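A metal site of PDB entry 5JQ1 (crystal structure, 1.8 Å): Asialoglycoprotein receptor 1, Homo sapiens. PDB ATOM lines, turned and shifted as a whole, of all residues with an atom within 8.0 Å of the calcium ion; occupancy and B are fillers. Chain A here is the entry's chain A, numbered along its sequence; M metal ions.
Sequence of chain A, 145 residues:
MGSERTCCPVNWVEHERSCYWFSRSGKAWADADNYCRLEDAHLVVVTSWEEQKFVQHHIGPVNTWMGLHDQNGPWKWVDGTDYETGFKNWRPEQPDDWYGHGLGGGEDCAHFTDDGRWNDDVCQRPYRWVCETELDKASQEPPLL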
ATOM      1  N   HIS A  15     -17.764   6.279  13.853  1.00  0.00           N
ATOM      2  CA  HIS A  15     -18.212   5.814  12.559  1.00  0.00           C
ATOM      3  C   HIS A  15     -19.392   6.662  12.101  1.00  0.00           C
ATOM      4  O   HIS A  15     -20.405   6.715  12.801  1.00  0.00           O
ATOM      5  CB  HIS A  15     -18.588   4.313  12.585  1.00  0.00           C
ATOM      6  CG  HIS A  15     -19.134   3.804  11.277  1.00  0.00           C
ATOM      7  ND1 HIS A  15     -18.287   3.447  10.243  1.00  0.00           N
ATOM      8  CD2 HIS A  15     -20.410   3.640  10.877  1.00  0.00           C
ATOM      9  CE1 HIS A  15     -19.063   3.077   9.246  1.00  0.00           C
ATOM     10  NE2 HIS A  15     -20.350   3.155   9.574  1.00  0.00           N
ATOM     11  N   GLU A  16     -19.235   7.327  10.934  1.00  0.00           N
ATOM     12  CA  GLU A  16     -20.292   8.128  10.287  1.00  0.00           C
ATOM     13  C   GLU A  16     -21.049   9.042  11.277  1.00  0.00           C
ATOM     14  O   GLU A  16     -22.270   8.916  11.423  1.00  0.00           O
ATOM     15  CB  GLU A  16     -21.264   7.209   9.510  1.00  0.00           C
ATOM     16  CG  GLU A  16     -20.655   6.521   8.290  1.00  0.00           C
ATOM     17  CD  GLU A  16     -20.271   7.444   7.150  1.00  0.00           C
ATOM     18  OE1 GLU A  16     -21.002   8.420   6.879  1.00  0.00           O
ATOM     19  OE2 GLU A  16     -19.216   7.182   6.508  1.00  0.00           O
ATOM     20  N   SER A  18     -21.247   8.950  14.489  1.00  0.00           N
ATOM     21  CA  SER A  18     -21.695   8.272  15.701  1.00  0.00           C
ATOM     22  C   SER A  18     -20.487   7.673  16.437  1.00  0.00           C
ATOM     23  O   SER A  18     -19.446   7.402  15.828  1.00  0.00           O
ATOM     24  CB  SER A  18     -22.720   7.196  15.361  1.00  0.00           C
ATOM     25  OG  SER A  18     -24.033   7.713  15.484  1.00  0.00           O
ATOM     26  N   CYS A  19     -20.620   7.532  17.771  1.00  0.00           N
ATOM     27  CA  CYS A  19     -19.596   6.946  18.655  1.00  0.00           C
ATOM     28  C   CYS A  19     -20.193   5.660  19.193  1.00  0.00           C
ATOM     29  O   CYS A  19     -21.335   5.690  19.636  1.00  0.00           O
ATOM     30  CB  CYS A  19     -19.269   7.898  19.800  1.00  0.00           C
ATOM     31  SG  CYS A  19     -18.740   9.548  19.261  1.00  0.00           S
ATOM     32  N   TYR A  20     -19.432   4.554  19.171  1.00  0.00           N
ATOM     33  CA  TYR A  20     -19.895   3.242  19.628  1.00  0.00           C
ATOM     34  C   TYR A  20     -18.963   2.650  20.663  1.00  0.00           C
ATOM     35  O   TYR A  20     -17.732   2.787  20.565  1.00  0.00           O
ATOM     36  CB  TYR A  20     -19.999   2.249  18.430  1.00  0.00           C
ATOM     37  CG  TYR A  20     -20.824   2.757  17.281  1.00  0.00           C
ATOM     38  CD1 TYR A  20     -20.289   3.624  16.336  1.00  0.00           C
ATOM     39  CD2 TYR A  20     -22.132   2.306  17.078  1.00  0.00           C
ATOM     40  CE1 TYR A  20     -21.055   4.086  15.261  1.00  0.00           C
ATOM     41  CE2 TYR A  20     -22.901   2.745  16.011  1.00  0.00           C
ATOM     42  CZ  TYR A  20     -22.348   3.627  15.086  1.00  0.00           C
ATOM     43  OH  TYR A  20     -23.116   4.090  14.052  1.00  0.00           O
ATOM     44  N   HIS A  42     -27.207   5.359  24.266  1.00  0.00           N
ATOM     45  CA  HIS A  42     -28.388   4.517  24.165  1.00  0.00           C
ATOM     46  C   HIS A  42     -27.908   3.247  23.499  1.00  0.00           C
ATOM     47  O   HIS A  42     -26.879   3.274  22.826  1.00  0.00           O
ATOM     48  CB  HIS A  42     -29.498   5.213  23.306  1.00  0.00           C
ATOM     49  CG  HIS A  42     -29.054   5.635  21.944  1.00  0.00           C
ATOM     50  ND1 HIS A  42     -28.989   4.732  20.891  1.00  0.00           N
ATOM     51  CD2 HIS A  42     -28.618   6.847  21.505  1.00  0.00           C
ATOM     52  CE1 HIS A  42     -28.558   5.417  19.838  1.00  0.00           C
ATOM     53  NE2 HIS A  42     -28.318   6.695  20.160  1.00  0.00           N
ATOM     54  N   LEU A  43     -28.628   2.142  23.670  1.00  0.00           N
ATOM     55  CA  LEU A  43     -28.318   0.888  22.983  1.00  0.00           C
ATOM     56  C   LEU A  43     -28.356   1.165  21.455  1.00  0.00           C
ATOM     57  O   LEU A  43     -29.221   1.920  21.005  1.00  0.00           O
ATOM     58  CB  LEU A  43     -29.323  -0.196  23.380  1.00  0.00           C
ATOM     59  CG  LEU A  43     -29.104  -0.883  24.731  1.00  0.00           C
ATOM     60  CD1 LEU A  43     -30.338  -1.681  25.113  1.00  0.00           C
ATOM     61  CD2 LEU A  43     -27.831  -1.788  24.716  1.00  0.00           C
ATOM     62  N   VAL A  44     -27.385   0.613  20.686  1.00  0.00           N
ATOM     63  CA  VAL A  44     -27.199   0.913  19.256  1.00  0.00           C
ATOM     64  C   VAL A  44     -28.551   0.887  18.488  1.00  0.00           C
ATOM     65  O   VAL A  44     -29.371   0.009  18.680  1.00  0.00           O
ATOM     66  CB  VAL A  44     -26.106   0.024  18.593  1.00  0.00           C
ATOM     67  CG1 VAL A  44     -26.479  -1.450  18.594  1.00  0.00           C
ATOM     68  CG2 VAL A  44     -25.728   0.518  17.185  1.00  0.00           C
ATOM     69  N   VAL A  45     -28.771   1.902  17.657  1.00  0.00           N
ATOM     70  CA  VAL A  45     -29.974   2.025  16.815  1.00  0.00           C
ATOM     71  C   VAL A  45     -29.427   1.952  15.379  1.00  0.00           C
ATOM     72  O   VAL A  45     -28.571   2.773  15.025  1.00  0.00           O
ATOM     73  CB  VAL A  45     -30.756   3.341  17.125  1.00  0.00           C
ATOM     74  CG1 VAL A  45     -31.832   3.606  16.068  1.00  0.00           C
ATOM     75  CG2 VAL A  45     -31.360   3.293  18.534  1.00  0.00           C
ATOM     76  N   VAL A  46     -29.816   0.912  14.629  1.00  0.00           N
ATOM     77  CA  VAL A  46     -29.286   0.627  13.279  1.00  0.00           C
ATOM     78  C   VAL A  46     -30.242   1.179  12.220  1.00  0.00           C
ATOM     79  O   VAL A  46     -31.402   0.773  12.201  1.00  0.00           O
ATOM     80  CB  VAL A  46     -28.971  -0.887  13.087  1.00  0.00           C
ATOM     81  CG1 VAL A  46     -28.305  -1.155  11.717  1.00  0.00           C
ATOM     82  CG2 VAL A  46     -28.087  -1.424  14.225  1.00  0.00           C
ATOM     83  N   THR A  47     -29.774   2.125  11.365  1.00  0.00           N
ATOM     84  CA  THR A  47     -30.680   2.752  10.389  1.00  0.00           C
ATOM     85  C   THR A  47     -30.238   2.579   8.935  1.00  0.00           C
ATOM     86  O   THR A  47     -30.885   3.145   8.049  1.00  0.00           O
ATOM     87  CB  THR A  47     -30.917   4.246  10.736  1.00  0.00           C
ATOM     88  OG1 THR A  47     -29.659   4.921  10.849  1.00  0.00           O
ATOM     89  CG2 THR A  47     -31.729   4.416  12.019  1.00  0.00           C
ATOM     90  N   SER A  48     -29.211   1.765   8.678  1.00  0.00           N
ATOM     91  CA  SER A  48     -28.708   1.536   7.308  1.00  0.00           C
ATOM     92  C   SER A  48     -27.903   0.238   7.201  1.00  0.00           C
ATOM     93  O   SER A  48     -27.427  -0.279   8.219  1.00  0.00           O
ATOM     94  CB  SER A  48     -27.833   2.712   6.857  1.00  0.00           C
ATOM     95  OG  SER A  48     -26.608   2.790   7.582  1.00  0.00           O
ATOM     96  N   GLU A  51     -24.262   0.808   8.400  1.00  0.00           N
ATOM     97  CA  GLU A  51     -24.139   0.817   9.861  1.00  0.00           C
ATOM     98  C   GLU A  51     -24.231  -0.620  10.373  1.00  0.00           C
ATOM     99  O   GLU A  51     -23.488  -0.988  11.294  1.00  0.00           O
ATOM    100  CB  GLU A  51     -25.234   1.685  10.515  1.00  0.00           C
ATOM    101  CG  GLU A  51     -25.066   1.768  12.029  1.00  0.00           C
ATOM    102  CD  GLU A  51     -25.977   2.733  12.770  1.00  0.00           C
ATOM    103  OE1 GLU A  51     -25.618   3.118  13.904  1.00  0.00           O
ATOM    104  OE2 GLU A  51     -27.049   3.099  12.241  1.00  0.00           O
ATOM    105  N   VAL A  55     -21.293  -2.503  12.598  1.00  0.00           N
ATOM    106  CA  VAL A  55     -21.544  -3.136  13.906  1.00  0.00           C
ATOM    107  C   VAL A  55     -21.112  -4.622  13.876  1.00  0.00           C
ATOM    108  O   VAL A  55     -20.361  -5.073  14.737  1.00  0.00           O
ATOM    109  CB  VAL A  55     -23.001  -2.940  14.442  1.00  0.00           C
ATOM    110  CG1 VAL A  55     -23.272  -3.808  15.674  1.00  0.00           C
ATOM    111  CG2 VAL A  55     -23.289  -1.473  14.773  1.00  0.00           C
ATOM    112  N   TRP A  77     -37.619   1.628  18.694  1.00  0.00           N
ATOM    113  CA  TRP A  77     -36.180   1.881  18.869  1.00  0.00           C
ATOM    114  C   TRP A  77     -36.101   2.758  20.129  1.00  0.00           C
ATOM    115  O   TRP A  77     -36.974   3.607  20.311  1.00  0.00           O
ATOM    116  CB  TRP A  77     -35.595   2.599  17.629  1.00  0.00           C
ATOM    117  CG  TRP A  77     -35.435   1.683  16.445  1.00  0.00           C
ATOM    118  CD1 TRP A  77     -36.218   1.628  15.327  1.00  0.00           C
ATOM    119  CD2 TRP A  77     -34.382   0.724  16.250  1.00  0.00           C
ATOM    120  NE1 TRP A  77     -35.750   0.647  14.477  1.00  0.00           N
ATOM    121  CE2 TRP A  77     -34.622   0.084  15.013  1.00  0.00           C
ATOM    122  CE3 TRP A  77     -33.278   0.303  17.039  1.00  0.00           C
ATOM    123  CZ2 TRP A  77     -33.774  -0.903  14.503  1.00  0.00           C
ATOM    124  CZ3 TRP A  77     -32.436  -0.690  16.534  1.00  0.00           C
ATOM    125  CH2 TRP A  77     -32.691  -1.294  15.286  1.00  0.00           C
ATOM    126  N   ASP A  79     -34.394   5.312  21.050  1.00  0.00           N
ATOM    127  CA  ASP A  79     -34.292   6.772  20.858  1.00  0.00           C
ATOM    128  C   ASP A  79     -35.489   7.392  20.062  1.00  0.00           C
ATOM    129  O   ASP A  79     -35.372   8.495  19.539  1.00  0.00           O
ATOM    130  CB  ASP A  79     -32.941   7.114  20.198  1.00  0.00           C
ATOM    131  CG  ASP A  79     -32.854   6.725  18.725  1.00  0.00           C
ATOM    132  OD1 ASP A  79     -33.726   5.940  18.259  1.00  0.00           O
ATOM    133  OD2 ASP A  79     -31.912   7.196  18.052  1.00  0.00           O
ATOM    134  N   THR A  81     -36.567   6.559  17.086  1.00  0.00           N
ATOM    135  CA  THR A  81     -36.461   6.358  15.621  1.00  0.00           C
ATOM    136  C   THR A  81     -37.657   5.484  15.222  1.00  0.00           C
ATOM    137  O   THR A  81     -37.950   4.508  15.913  1.00  0.00           O
ATOM    138  CB  THR A  81     -35.125   5.676  15.252  1.00  0.00           C
ATOM    139  OG1 THR A  81     -34.039   6.529  15.613  1.00  0.00           O
ATOM    140  CG2 THR A  81     -35.009   5.320  13.755  1.00  0.00           C
ATOM    141  N   GLU A 132     -24.295   3.594  21.782  1.00  0.00           N
ATOM    142  CA  GLU A 132     -24.115   4.537  20.692  1.00  0.00           C
ATOM    143  C   GLU A 132     -24.515   5.933  21.146  1.00  0.00           C
ATOM    144  O   GLU A 132     -25.495   6.084  21.874  1.00  0.00           O
ATOM    145  CB  GLU A 132     -24.954   4.106  19.468  1.00  0.00           C
ATOM    146  CG  GLU A 132     -24.758   5.034  18.270  1.00  0.00           C
ATOM    147  CD  GLU A 132     -25.664   4.843  17.064  1.00  0.00           C
ATOM    148  OE1 GLU A 132     -26.672   4.123  17.178  1.00  0.00           O
ATOM    149  OE2 GLU A 132     -25.377   5.464  16.018  1.00  0.00           O
ATOM    150  N   THR A 133     -23.765   6.935  20.700  1.00  0.00           N
ATOM    151  CA  THR A 133     -24.098   8.337  20.925  1.00  0.00           C
ATOM    152  C   THR A 133     -23.840   9.069  19.594  1.00  0.00           C
ATOM    153  O   THR A 133     -23.003   8.620  18.802  1.00  0.00           O
ATOM    154  CB  THR A 133     -23.457   8.915  22.193  1.00  0.00           C
ATOM    155  OG1 THR A 133     -24.111  10.160  22.479  1.00  0.00           O
ATOM    156  CG2 THR A 133     -21.953   9.100  22.098  1.00  0.00           C
ATOM    157  N   GLU A 134     -24.624  10.115  19.312  1.00  0.00           N
ATOM    158  CA  GLU A 134     -24.469  10.865  18.047  1.00  0.00           C
ATOM    159  C   GLU A 134     -23.666  12.121  18.279  1.00  0.00           C
ATOM    160  O   GLU A 134     -23.851  12.813  19.289  1.00  0.00           O
ATOM    161  CB  GLU A 134     -25.834  11.222  17.416  1.00  0.00           C
ATOM    162  CG  GLU A 134     -26.695  10.037  16.957  1.00  0.00           C
ATOM    163  CD  GLU A 134     -27.311   9.202  18.060  1.00  0.00           C
ATOM    164  OE1 GLU A 134     -27.117   7.972  18.028  1.00  0.00           O
ATOM    165  OE2 GLU A 134     -27.888   9.778  19.015  1.00  0.00           O
HETATM  166 CA    CA M   1     -27.248   4.661  14.663  1.00  0.00          CA
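OE1 of Glu 51 lies close to OH of Tyr 20 (2.7 Å). The backbone NH of Thr 47 lies close to the side-chain carboxylate of Glu 51 (3.0 Å). N of Glu 51 lies within hydrogen-bond range of OG of Ser 48 (3.2 Å). OE2 of Glu 132 lies close to OH of Tyr 20, at 3.3 Å. OE2 of Glu 132 lies close to OG of Ser 18 (2.7 Å). The backbone carbonyl oxygen (O) of His 42 is in hydrogen-bond range of the backbone NH (N) of Glu 132 (2.8 Å).
Three residues have an atom within 4 Å of the calcium ion: Val 45, Glu 51 and Glu 132. The nearest printed residue that does not touch the calcium ion is Tyr 20 (4.2 Å).
The calcium ion is bound by the backbone carbonyl oxygen (O) of Val 45, at 2.3 Å. OE1 of Glu 51 is bound to the calcium ion (2.4 Å). The side-chain carboxylate (OE2) of Glu 132 binds the calcium ion, 2.4 Å away. OE1 of Glu 132 binds the calcium ion. The calcium ion is bound by OE2 of Glu 51, at 2.9 Å.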
